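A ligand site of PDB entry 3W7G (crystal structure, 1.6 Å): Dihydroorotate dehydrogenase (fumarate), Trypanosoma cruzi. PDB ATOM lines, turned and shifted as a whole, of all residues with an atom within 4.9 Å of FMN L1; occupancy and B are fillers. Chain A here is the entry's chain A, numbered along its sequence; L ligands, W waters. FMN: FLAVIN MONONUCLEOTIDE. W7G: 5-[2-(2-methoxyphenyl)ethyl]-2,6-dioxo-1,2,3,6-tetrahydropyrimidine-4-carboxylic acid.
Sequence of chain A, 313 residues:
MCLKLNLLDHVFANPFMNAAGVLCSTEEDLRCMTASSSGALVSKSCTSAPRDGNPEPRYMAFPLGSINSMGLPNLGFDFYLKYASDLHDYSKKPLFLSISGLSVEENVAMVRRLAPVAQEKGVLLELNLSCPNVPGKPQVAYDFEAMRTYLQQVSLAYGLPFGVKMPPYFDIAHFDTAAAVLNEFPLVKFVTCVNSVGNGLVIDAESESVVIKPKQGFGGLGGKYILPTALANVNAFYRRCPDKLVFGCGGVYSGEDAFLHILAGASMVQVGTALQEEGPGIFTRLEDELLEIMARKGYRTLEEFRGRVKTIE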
ATOM      1  N   ALA A  19     -10.327  16.903 -27.725  1.00  0.00           N
ATOM      2  CA  ALA A  19      -9.322  16.198 -28.515  1.00  0.00           C
ATOM      3  C   ALA A  19      -9.485  14.690 -28.305  1.00  0.00           C
ATOM      4  O   ALA A  19      -9.811  14.256 -27.205  1.00  0.00           O
ATOM      5  CB  ALA A  19      -7.951  16.632 -28.080  1.00  0.00           C
ATOM      6  N   ALA A  20      -9.327  13.917 -29.364  1.00  0.00           N
ATOM      7  CA  ALA A  20      -9.431  12.488 -29.205  1.00  0.00           C
ATOM      8  C   ALA A  20      -8.539  12.038 -28.080  1.00  0.00           C
ATOM      9  O   ALA A  20      -7.436  12.466 -27.917  1.00  0.00           O
ATOM     10  CB  ALA A  20      -9.108  11.770 -30.509  1.00  0.00           C
ATOM     11  N   GLY A  21      -9.039  11.116 -27.280  1.00  0.00           N
ATOM     12  CA  GLY A  21      -8.339  10.607 -26.146  1.00  0.00           C
ATOM     13  C   GLY A  21      -8.790  11.143 -24.826  1.00  0.00           C
ATOM     14  O   GLY A  21      -8.603  10.552 -23.795  1.00  0.00           O
ATOM     15  N   VAL A  22      -9.320  12.365 -24.842  1.00  0.00           N
ATOM     16  CA  VAL A  22      -9.714  13.030 -23.598  1.00  0.00           C
ATOM     17  C   VAL A  22     -11.230  13.061 -23.422  1.00  0.00           C
ATOM     18  O   VAL A  22     -11.876  13.435 -24.260  1.00  0.00           O
ATOM     19  CB  VAL A  22      -9.084  14.452 -23.520  1.00  0.00           C
ATOM     20  CG1 VAL A  22      -9.528  15.181 -22.289  1.00  0.00           C
ATOM     21  CG2 VAL A  22      -7.577  14.357 -23.601  1.00  0.00           C
ATOM     22  N   LYS A  44     -13.147   8.238 -28.452  1.00  0.00           N
ATOM     23  CA  LYS A  44     -11.821   7.749 -28.262  1.00  0.00           C
ATOM     24  C   LYS A  44     -11.338   6.931 -29.467  1.00  0.00           C
ATOM     25  O   LYS A  44     -12.012   5.990 -29.899  1.00  0.00           O
ATOM     26  CB  LYS A  44     -11.769   6.887 -27.011  1.00  0.00           C
ATOM     27  CG  LYS A  44     -10.410   6.219 -26.742  1.00  0.00           C
ATOM     28  CD  LYS A  44      -9.306   7.190 -26.440  1.00  0.00           C
ATOM     29  CE  LYS A  44      -7.976   6.536 -26.819  1.00  0.00           C
ATOM     30  NZ  LYS A  44      -7.471   6.288 -25.516  1.00  0.00           N
ATOM     31  N   SER A  45     -10.142   7.229 -29.935  1.00  0.00           N
ATOM     32  CA  SER A  45      -9.493   6.439 -31.031  1.00  0.00           C
ATOM     33  C   SER A  45      -9.594   4.966 -30.673  1.00  0.00           C
ATOM     34  O   SER A  45      -9.208   4.519 -29.607  1.00  0.00           O
ATOM     35  CB  SER A  45      -8.049   6.775 -31.294  1.00  0.00           C
ATOM     36  OG  SER A  45      -7.974   8.142 -31.660  1.00  0.00           O
ATOM     37  N   TYR A  59      -0.078   8.773 -17.956  1.00  0.00           N
ATOM     38  CA  TYR A  59      -0.361  10.185 -18.200  1.00  0.00           C
ATOM     39  C   TYR A  59       0.016  10.973 -16.968  1.00  0.00           C
ATOM     40  O   TYR A  59      -0.351  10.589 -15.855  1.00  0.00           O
ATOM     41  CB  TYR A  59      -1.851  10.407 -18.502  1.00  0.00           C
ATOM     42  CG  TYR A  59      -2.351  11.866 -18.515  1.00  0.00           C
ATOM     43  CD1 TYR A  59      -2.206  12.667 -19.659  1.00  0.00           C
ATOM     44  CD2 TYR A  59      -2.797  12.498 -17.366  1.00  0.00           C
ATOM     45  CE1 TYR A  59      -2.628  14.001 -19.698  1.00  0.00           C
ATOM     46  CE2 TYR A  59      -3.127  13.844 -17.358  1.00  0.00           C
ATOM     47  CZ  TYR A  59      -3.093  14.579 -18.528  1.00  0.00           C
ATOM     48  OH  TYR A  59      -3.449  15.909 -18.567  1.00  0.00           O
ATOM     49  N   SER A  66       1.364  18.244 -20.550  1.00  0.00           N
ATOM     50  CA  SER A  66       1.207  16.867 -20.178  1.00  0.00           C
ATOM     51  C   SER A  66       2.145  15.972 -21.067  1.00  0.00           C
ATOM     52  O   SER A  66       2.619  16.356 -22.121  1.00  0.00           O
ATOM     53  CB  SER A  66      -0.229  16.433 -20.391  1.00  0.00           C
ATOM     54  OG  SER A  66      -0.573  16.400 -21.794  1.00  0.00           O
ATOM     55  N   ASN A  68       2.166  11.632 -22.175  1.00  0.00           N
ATOM     56  CA  ASN A  68       1.372  10.407 -22.129  1.00  0.00           C
ATOM     57  C   ASN A  68       1.997   9.375 -23.043  1.00  0.00           C
ATOM     58  O   ASN A  68       2.385   9.606 -24.165  1.00  0.00           O
ATOM     59  CB  ASN A  68      -0.099  10.571 -22.472  1.00  0.00           C
ATOM     60  CG  ASN A  68      -0.396  10.532 -23.933  1.00  0.00           C
ATOM     61  OD1 ASN A  68      -0.552   9.432 -24.519  1.00  0.00           O
ATOM     62  ND2 ASN A  68      -0.522  11.689 -24.554  1.00  0.00           N
ATOM     63  N   MET A  70      -0.229   6.249 -23.411  1.00  0.00           N
ATOM     64  CA  MET A  70      -1.365   5.538 -22.941  1.00  0.00           C
ATOM     65  C   MET A  70      -1.403   4.097 -23.406  1.00  0.00           C
ATOM     66  O   MET A  70      -1.995   3.229 -22.752  1.00  0.00           O
ATOM     67  CB  MET A  70      -2.640   6.225 -23.389  1.00  0.00           C
ATOM     68  CG  MET A  70      -2.880   7.588 -22.930  1.00  0.00           C
ATOM     69  SD  MET A  70      -2.890   7.840 -21.171  1.00  0.00           S
ATOM     70  CE  MET A  70      -4.387   7.097 -20.754  1.00  0.00           C
ATOM     71  N   LEU A  72      -2.961   3.295 -26.320  1.00  0.00           N
ATOM     72  CA  LEU A  72      -4.236   3.215 -27.075  1.00  0.00           C
ATOM     73  C   LEU A  72      -5.299   2.378 -26.323  1.00  0.00           C
ATOM     74  O   LEU A  72      -5.920   1.498 -26.949  1.00  0.00           O
ATOM     75  CB  LEU A  72      -3.968   2.715 -28.492  1.00  0.00           C
ATOM     76  CG  LEU A  72      -5.024   2.869 -29.568  1.00  0.00           C
ATOM     77  CD1 LEU A  72      -5.699   4.187 -29.469  1.00  0.00           C
ATOM     78  CD2 LEU A  72      -4.387   2.632 -30.959  1.00  0.00           C
ATOM     79  N   SER A  98     -13.187   8.624 -33.934  1.00  0.00           N
ATOM     80  CA  SER A  98     -11.805   8.490 -34.320  1.00  0.00           C
ATOM     81  C   SER A  98     -11.458   7.027 -34.365  1.00  0.00           C
ATOM     82  O   SER A  98     -11.795   6.247 -33.477  1.00  0.00           O
ATOM     83  CB  SER A  98     -10.919   9.164 -33.254  1.00  0.00           C
ATOM     84  OG  SER A  98      -9.540   8.905 -33.562  1.00  0.00           O
ATOM     85  N   GLU A 126     -12.725  10.587 -38.124  1.00  0.00           N
ATOM     86  CA  GLU A 126     -11.355  11.111 -37.998  1.00  0.00           C
ATOM     87  C   GLU A 126     -10.413   9.896 -37.934  1.00  0.00           C
ATOM     88  O   GLU A 126     -10.384   9.153 -36.982  1.00  0.00           O
ATOM     89  CB  GLU A 126     -11.237  12.076 -36.787  1.00  0.00           C
ATOM     90  CG  GLU A 126      -9.841  12.751 -36.661  1.00  0.00           C
ATOM     91  CD  GLU A 126      -9.722  13.718 -35.426  1.00  0.00           C
ATOM     92  OE1 GLU A 126      -9.388  13.207 -34.317  1.00  0.00           O
ATOM     93  OE2 GLU A 126      -9.911  14.982 -35.492  1.00  0.00           O
ATOM     94  N   ASN A 128      -6.808   8.490 -37.373  1.00  0.00           N
ATOM     95  CA  ASN A 128      -5.534   8.854 -36.750  1.00  0.00           C
ATOM     96  C   ASN A 128      -4.365   8.314 -37.519  1.00  0.00           C
ATOM     97  O   ASN A 128      -4.142   7.112 -37.552  1.00  0.00           O
ATOM     98  CB  ASN A 128      -5.476   8.359 -35.318  1.00  0.00           C
ATOM     99  CG  ASN A 128      -4.255   8.885 -34.587  1.00  0.00           C
ATOM    100  OD1 ASN A 128      -3.681   9.889 -34.899  1.00  0.00           O
ATOM    101  ND2 ASN A 128      -3.875   8.198 -33.553  1.00  0.00           N
ATOM    102  N   LYS A 165      -6.099  12.916 -38.530  1.00  0.00           N
ATOM    103  CA  LYS A 165      -5.393  13.504 -37.368  1.00  0.00           C
ATOM    104  C   LYS A 165      -3.916  13.347 -37.681  1.00  0.00           C
ATOM    105  O   LYS A 165      -3.409  12.246 -37.813  1.00  0.00           O
ATOM    106  CB  LYS A 165      -5.735  12.725 -36.148  1.00  0.00           C
ATOM    107  CG  LYS A 165      -5.088  13.215 -34.818  1.00  0.00           C
ATOM    108  CD  LYS A 165      -5.614  14.562 -34.347  1.00  0.00           C
ATOM    109  CE  LYS A 165      -5.171  14.957 -32.973  1.00  0.00           C
ATOM    110  NZ  LYS A 165      -5.780  14.118 -31.948  1.00  0.00           N
ATOM    111  N   VAL A 194      -2.765  19.488 -34.233  1.00  0.00           N
ATOM    112  CA  VAL A 194      -1.862  18.337 -34.280  1.00  0.00           C
ATOM    113  C   VAL A 194      -2.118  17.381 -33.146  1.00  0.00           C
ATOM    114  O   VAL A 194      -2.730  17.732 -32.112  1.00  0.00           O
ATOM    115  CB  VAL A 194      -0.341  18.773 -34.105  1.00  0.00           C
ATOM    116  CG1 VAL A 194       0.036  19.623 -35.327  1.00  0.00           C
ATOM    117  CG2 VAL A 194      -0.107  19.580 -32.844  1.00  0.00           C
ATOM    118  N   ASN A 195      -1.664  16.157 -33.358  1.00  0.00           N
ATOM    119  CA  ASN A 195      -1.453  15.162 -32.318  1.00  0.00           C
ATOM    120  C   ASN A 195      -0.228  15.589 -31.437  1.00  0.00           C
ATOM    121  O   ASN A 195       0.355  16.660 -31.692  1.00  0.00           O
ATOM    122  CB  ASN A 195      -1.314  13.731 -32.926  1.00  0.00           C
ATOM    123  CG  ASN A 195      -1.848  12.637 -32.022  1.00  0.00           C
ATOM    124  OD1 ASN A 195      -1.587  12.621 -30.826  1.00  0.00           O
ATOM    125  ND2 ASN A 195      -2.647  11.776 -32.539  1.00  0.00           N
ATOM    126  N   SER A 196       0.140  14.764 -30.432  1.00  0.00           N
ATOM    127  CA  SER A 196       1.201  15.185 -29.559  1.00  0.00           C
ATOM    128  C   SER A 196       2.488  15.375 -30.226  1.00  0.00           C
ATOM    129  O   SER A 196       2.816  14.833 -31.248  1.00  0.00           O
ATOM    130  CB  SER A 196       1.584  14.113 -28.561  1.00  0.00           C
ATOM    131  OG  SER A 196       0.663  13.173 -28.317  1.00  0.00           O
ATOM    132  N   GLY A 222       1.686  17.383 -24.759  1.00  0.00           N
ATOM    133  CA  GLY A 222       0.570  18.306 -25.047  1.00  0.00           C
ATOM    134  C   GLY A 222       0.656  19.511 -24.189  1.00  0.00           C
ATOM    135  O   GLY A 222       1.470  19.571 -23.207  1.00  0.00           O
ATOM    136  N   GLY A 223      -0.232  20.443 -24.438  1.00  0.00           N
ATOM    137  CA  GLY A 223      -0.402  21.587 -23.603  1.00  0.00           C
ATOM    138  C   GLY A 223       0.417  22.802 -24.005  1.00  0.00           C
ATOM    139  O   GLY A 223       0.704  23.010 -25.182  1.00  0.00           O
ATOM    140  N   ILE A 226       3.346  23.073 -26.619  1.00  0.00           N
ATOM    141  CA  ILE A 226       3.202  22.791 -28.020  1.00  0.00           C
ATOM    142  C   ILE A 226       2.379  23.812 -28.825  1.00  0.00           C
ATOM    143  O   ILE A 226       2.183  23.640 -30.017  1.00  0.00           O
ATOM    144  CB  ILE A 226       2.678  21.318 -28.231  1.00  0.00           C
ATOM    145  CG1 ILE A 226       1.148  21.215 -28.102  1.00  0.00           C
ATOM    146  CG2 ILE A 226       3.407  20.297 -27.391  1.00  0.00           C
ATOM    147  CD1 ILE A 226       0.547  19.969 -28.722  1.00  0.00           C
ATOM    148  N   CYS A 249      -5.607  21.720 -33.021  1.00  0.00           N
ATOM    149  CA  CYS A 249      -5.502  21.026 -31.722  1.00  0.00           C
ATOM    150  C   CYS A 249      -4.100  21.280 -31.208  1.00  0.00           C
ATOM    151  O   CYS A 249      -3.163  21.134 -31.969  1.00  0.00           O
ATOM    152  CB  CYS A 249      -5.736  19.547 -31.913  1.00  0.00           C
ATOM    153  SG  CYS A 249      -5.832  18.636 -30.353  1.00  0.00           S
ATOM    154  N   GLY A 250      -3.951  21.767 -29.982  1.00  0.00           N
ATOM    155  CA  GLY A 250      -2.632  21.801 -29.295  1.00  0.00           C
ATOM    156  C   GLY A 250      -2.535  23.084 -28.529  1.00  0.00           C
ATOM    157  O   GLY A 250      -2.568  24.189 -29.082  1.00  0.00           O
ATOM    158  N   GLY A 251      -2.382  22.949 -27.216  1.00  0.00           N
ATOM    159  CA  GLY A 251      -2.090  24.118 -26.433  1.00  0.00           C
ATOM    160  C   GLY A 251      -3.204  25.085 -26.164  1.00  0.00           C
ATOM    161  O   GLY A 251      -2.960  26.225 -25.759  1.00  0.00           O
ATOM    162  N   VAL A 252      -4.446  24.660 -26.361  1.00  0.00           N
ATOM    163  CA  VAL A 252      -5.569  25.585 -26.064  1.00  0.00           C
ATOM    164  C   VAL A 252      -5.944  25.505 -24.613  1.00  0.00           C
ATOM    165  O   VAL A 252      -6.476  24.479 -24.181  1.00  0.00           O
ATOM    166  CB  VAL A 252      -6.813  25.302 -26.967  1.00  0.00           C
ATOM    167  CG1 VAL A 252      -8.027  26.174 -26.660  1.00  0.00           C
ATOM    168  CG2 VAL A 252      -6.401  25.433 -28.431  1.00  0.00           C
ATOM    169  N   GLN A 270      -9.923  21.909 -31.069  1.00  0.00           N
ATOM    170  CA  GLN A 270      -9.997  20.795 -30.108  1.00  0.00           C
ATOM    171  C   GLN A 270      -9.126  21.116 -28.851  1.00  0.00           C
ATOM    172  O   GLN A 270      -8.094  21.812 -28.920  1.00  0.00           O
ATOM    173  CB  GLN A 270      -9.469  19.516 -30.755  1.00  0.00           C
ATOM    174  CG  GLN A 270     -10.042  19.239 -32.091  1.00  0.00           C
ATOM    175  CD  GLN A 270      -9.699  17.884 -32.627  1.00  0.00           C
ATOM    176  OE1 GLN A 270      -8.666  17.290 -32.246  1.00  0.00           O
ATOM    177  NE2 GLN A 270     -10.481  17.364 -33.542  1.00  0.00           N
ATOM    178  N   VAL A 271      -9.569  20.537 -27.746  1.00  0.00           N
ATOM    179  CA  VAL A 271      -9.017  20.776 -26.428  1.00  0.00           C
ATOM    180  C   VAL A 271      -8.667  19.451 -25.755  1.00  0.00           C
ATOM    181  O   VAL A 271      -9.592  18.661 -25.492  1.00  0.00           O
ATOM    182  CB  VAL A 271      -9.966  21.647 -25.525  1.00  0.00           C
ATOM    183  CG1 VAL A 271      -9.210  22.083 -24.287  1.00  0.00           C
ATOM    184  CG2 VAL A 271     -10.517  22.865 -26.338  1.00  0.00           C
ATOM    185  N   GLY A 272      -7.352  19.207 -25.517  1.00  0.00           N
ATOM    186  CA  GLY A 272      -6.898  17.952 -24.900  1.00  0.00           C
ATOM    187  C   GLY A 272      -6.500  18.211 -23.453  1.00  0.00           C
ATOM    188  O   GLY A 272      -7.315  18.105 -22.544  1.00  0.00           O
ATOM    189  N   THR A 273      -5.193  18.462 -23.248  1.00  0.00           N
ATOM    190  CA  THR A 273      -4.650  18.627 -21.891  1.00  0.00           C
ATOM    191  C   THR A 273      -5.477  19.541 -20.993  1.00  0.00           C
ATOM    192  O   THR A 273      -5.802  19.198 -19.884  1.00  0.00           O
ATOM    193  CB  THR A 273      -3.229  19.149 -22.004  1.00  0.00           C
ATOM    194  OG1 THR A 273      -2.393  18.194 -22.715  1.00  0.00           O
ATOM    195  CG2 THR A 273      -2.608  19.304 -20.628  1.00  0.00           C
ATOM    196  N   ALA A 274      -5.846  20.671 -21.505  1.00  0.00           N
ATOM    197  CA  ALA A 274      -6.556  21.627 -20.678  1.00  0.00           C
ATOM    198  C   ALA A 274      -7.914  21.113 -20.231  1.00  0.00           C
ATOM    199  O   ALA A 274      -8.343  21.381 -19.117  1.00  0.00           O
ATOM    200  CB  ALA A 274      -6.729  22.976 -21.365  1.00  0.00           C
HETATM  201  N1  FMN L   1      -4.959  11.681 -30.090  1.00  0.00           N
HETATM  202  C2  FMN L   1      -5.566  10.781 -30.928  1.00  0.00           C
HETATM  203  O2  FMN L   1      -5.810  11.185 -32.108  1.00  0.00           O
HETATM  204  N3  FMN L   1      -6.054   9.622 -30.500  1.00  0.00           N
HETATM  205  C4  FMN L   1      -5.926   9.238 -29.204  1.00  0.00           C
HETATM  206  O4  FMN L   1      -6.380   8.154 -28.770  1.00  0.00           O
HETATM  207  C4A FMN L   1      -5.312  10.100 -28.298  1.00  0.00           C
HETATM  208  N5  FMN L   1      -5.242   9.773 -26.973  1.00  0.00           N
HETATM  209  C5A FMN L   1      -4.749  10.715 -26.087  1.00  0.00           C
HETATM  210  C6  FMN L   1      -4.852  10.496 -24.730  1.00  0.00           C
HETATM  211  C7  FMN L   1      -4.406  11.422 -23.821  1.00  0.00           C
HETATM  212  C7M FMN L   1      -4.458  11.122 -22.311  1.00  0.00           C
HETATM  213  C8  FMN L   1      -3.919  12.690 -24.278  1.00  0.00           C
HETATM  214  C8M FMN L   1      -3.398  13.752 -23.357  1.00  0.00           C
HETATM  215  C9  FMN L   1      -3.860  12.919 -25.631  1.00  0.00           C
HETATM  216  C9A FMN L   1      -4.304  11.999 -26.569  1.00  0.00           C
HETATM  217  N10 FMN L   1      -4.251  12.236 -27.955  1.00  0.00           N
HETATM  218  C10 FMN L   1      -4.876  11.384 -28.809  1.00  0.00           C
HETATM  219  C1' FMN L   1      -3.786  13.511 -28.437  1.00  0.00           C
HETATM  220  C2' FMN L   1      -4.732  14.679 -28.289  1.00  0.00           C
HETATM  221  O2' FMN L   1      -5.870  14.385 -29.112  1.00  0.00           O
HETATM  222  C3' FMN L   1      -4.100  15.943 -28.748  1.00  0.00           C
HETATM  223  O3' FMN L   1      -3.771  15.840 -30.144  1.00  0.00           O
HETATM  224  C4' FMN L   1      -2.820  16.326 -27.984  1.00  0.00           C
HETATM  225  O4' FMN L   1      -2.991  16.076 -26.561  1.00  0.00           O
HETATM  226  C5' FMN L   1      -2.514  17.838 -28.165  1.00  0.00           C
HETATM  227  O5' FMN L   1      -3.541  18.716 -27.727  1.00  0.00           O
HETATM  228  P   FMN L   1      -3.447  19.475 -26.295  1.00  0.00           P
HETATM  229  O1P FMN L   1      -4.778  20.197 -26.159  1.00  0.00           O
HETATM  230  O2P FMN L   1      -2.215  20.340 -26.348  1.00  0.00           O
HETATM  231  O3P FMN L   1      -3.283  18.341 -25.231  1.00  0.00           O
HETATM  232  OAB W7G L   2      -0.319   6.788 -26.512  1.00  0.00           O
HETATM  233  CAO W7G L   2      -1.513   6.778 -27.024  1.00  0.00           C
HETATM  234  OAE W7G L   2      -2.394   5.976 -26.790  1.00  0.00           O
HETATM  235  CAR W7G L   2      -1.779   7.966 -27.865  1.00  0.00           C
HETATM  236  NAL W7G L   2      -1.431   9.159 -27.274  1.00  0.00           N
HETATM  237  CAT W7G L   2      -1.510  10.347 -27.889  1.00  0.00           C
HETATM  238  OAC W7G L   2      -1.142  11.427 -27.388  1.00  0.00           O
HETATM  239  NAM W7G L   2      -1.940  10.341 -29.186  1.00  0.00           N
HETATM  240  CAU W7G L   2      -2.312   9.167 -29.889  1.00  0.00           C
HETATM  241  OAD W7G L   2      -2.712   9.258 -31.043  1.00  0.00           O
HETATM  242  CAS W7G L   2      -2.238   7.984 -29.163  1.00  0.00           C
HETATM  243  CAK W7G L   2      -2.573   6.729 -29.808  1.00  0.00           C
HETATM  244  CAJ W7G L   2      -1.516   6.268 -30.863  1.00  0.00           C
HETATM  245  CAP W7G L   2      -0.211   5.990 -30.271  1.00  0.00           C
HETATM  246  CAH W7G L   2       0.834   6.966 -30.131  1.00  0.00           C
HETATM  247  CAF W7G L   2       2.070   6.641 -29.501  1.00  0.00           C
HETATM  248  CAG W7G L   2       2.334   5.383 -29.032  1.00  0.00           C
HETATM  249  CAI W7G L   2       1.373   4.419 -29.153  1.00  0.00           C
HETATM  250  CAQ W7G L   2       0.141   4.687 -29.791  1.00  0.00           C
HETATM  251  OAN W7G L   2      -0.870   3.797 -29.970  1.00  0.00           O
HETATM  252  CAA W7G L   2      -0.565   2.371 -29.607  1.00  0.00           C
HETATM  253  O   HOH W   1      -5.102  21.842 -23.987  1.00  0.00           O
HETATM  254  O   HOH W   2      -4.880   6.724 -26.616  1.00  0.00           O
HETATM  255  O   HOH W   3      -7.959  10.947 -33.972  1.00  0.00           O
HETATM  256  O   HOH W   4      -0.642  14.902 -26.004  1.00  0.00           O
HETATM  257  O   HOH W   5      -5.662  22.185 -27.707  1.00  0.00           O
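N of Thr 273 sits at hydrogen-bond distance from O3P of FMN L1 (2.8 Å).
The side-chain hydroxyl of Thr 273 sits at hydrogen-bond distance from an oxygen (O3P) of FMN L1.
The side-chain hydroxyl of Ser 45 sits at hydrogen-bond distance from a nitrogen (N3) of FMN L1 (2.7 Å).
The backbone NH (N) of Ala 20 sits at hydrogen-bond distance from an oxygen (O2') of FMN L1 (3.5 Å).
The backbone carbonyl oxygen of Ala 20 sits at hydrogen-bond distance from an oxygen (O2') of FMN L1, at 2.8 Å.
N of Gly 251 is in hydrogen-bond range of O2P of FMN L1, 2.8 Å away.
The backbone NH (N) of Gly 223 lies within hydrogen-bond range of an oxygen (O2P) of FMN L1 (2.8 Å).
The backbone NH (N) of Gly 272 is in hydrogen-bond range of an oxygen (O1P) of FMN L1.
NZ of Lys 165 lies within hydrogen-bond range of O2' of FMN L1.
O of Val 194 is in hydrogen-bond range of O3' of FMN L1.
The side-chain amide nitrogen of Asn 195 sits at hydrogen-bond distance from an oxygen (O2) of FMN L1 (3.2 Å).
The side-chain sulfur of Cys 249 is in hydrogen-bond range of an oxygen (O3') of FMN L1, 3.5 Å away.
OD1 of Asn 195 is in hydrogen-bond range of NAM of W7G L2, at 2.8 Å.
OD1 of Asn 68 lies within hydrogen-bond range of NAL of W7G L2, 2.9 Å away.
The side-chain amide nitrogen of Asn 128 is in hydrogen-bond range of an oxygen (OAD) of W7G L2, at 3.0 Å.
OAB of W7G L2 lies within hydrogen-bond range of N of Met 70, at 3.1 Å.
OG of Ser 196 sits at hydrogen-bond distance from OAC of W7G L2 (2.7 Å).
The backbone NH of Leu 72 lies within hydrogen-bond range of an oxygen (OAE) of W7G L2, 2.8 Å away.
CB of Ala 19 touches O2' of FMN L1, 3.2 Å away.
Gly 21 touches FMN L1 (CA to N5, 3.3 Å).
Lys 44 touches FMN L1 (CE to O4, 3.0 Å).
Tyr 59 touches FMN L1 (CE1 to C8M, 3.7 Å).
Asn 68 touches FMN L1 (ND2 to C8, 3.6 Å).
Met 70 touches FMN L1 (SD to C7M, 3.8 Å).
CG of Asn 128 touches O2 of FMN L1, 3.7 Å away.
CA of Gly 222 touches O2P of FMN L1 (3.7 Å).
CD1 of Ile 226 touches O2P of FMN L1, at 3.7 Å.
CA of Gly 250 touches O2P of FMN L1, 3.3 Å away.
Val 271 touches FMN L1 (C to O1P, 3.98 Å).
Hydrophobic or aromatic side chains within 4 Å of FMN L1: Ala 19, Ala 20, Tyr 59, Met 70 and Ile 226.
21 residues have an atom within 4 Å of FMN L1: Ala 19, Ala 20, Gly 21, Lys 44, Ser 45, Tyr 59, Asn 68, Met 70, Asn 128, Lys 165, Val 194, Asn 195, Gly 222, Gly 223, Ile 226, Cys 249, Gly 250, Gly 251, Val 271, Gly 272 and Thr 273.
The nearest printed residue that does not touch FMN L1 is Ser 196 (4.1 Å).
OG of Ser 45 is in hydrogen-bond range of OG of Ser 98.
N of Val 194 lies within hydrogen-bond range of O of Cys 249, 2.8 Å away.
N of Ala 19 lies within hydrogen-bond range of O of Val 271 (2.9 Å).
The side-chain amide oxygen (OD1) of Asn 128 lies within hydrogen-bond range of the side-chain amide nitrogen (ND2) of Asn 195 (3.2 Å).
The side-chain amide oxygen (OD1) of Asn 195 is in hydrogen-bond range of the side-chain hydroxyl (OG) of Ser 196, 3.4 Å away.
SG of Cys 249 sits at hydrogen-bond distance from OE1 of Gln 270, 3.7 Å away.
OD1 of Asn 68 sits close to N of Met 70 (3.4 Å).
N of Ser 66 lies within hydrogen-bond range of O of Gly 222, 3.0 Å away.
Water W4 lies within hydrogen-bond range of O4' of FMN L1 and OG of Ser 196.
Water W1 lies within hydrogen-bond range of an oxygen (O1P) of FMN L1 (2.7 Å), the backbone NH of Ala 274 (2.8 Å), the backbone carbonyl oxygen of Val 252 (3.0 Å) and the backbone NH of Thr 273 (3.5 Å).
Water W3 lies within hydrogen-bond range of OG of Ser 98, OE1 of Glu 126 and O2 of FMN L1.
Water W2 lies within hydrogen-bond range of OAE of W7G L2 (2.6 Å), NZ of Lys 44 (2.8 Å) and O4 of FMN L1 (3.0 Å).
A nitrogen (N3) of FMN L1 lies close to an oxygen (OAD) of W7G L2, 3.4 Å away.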
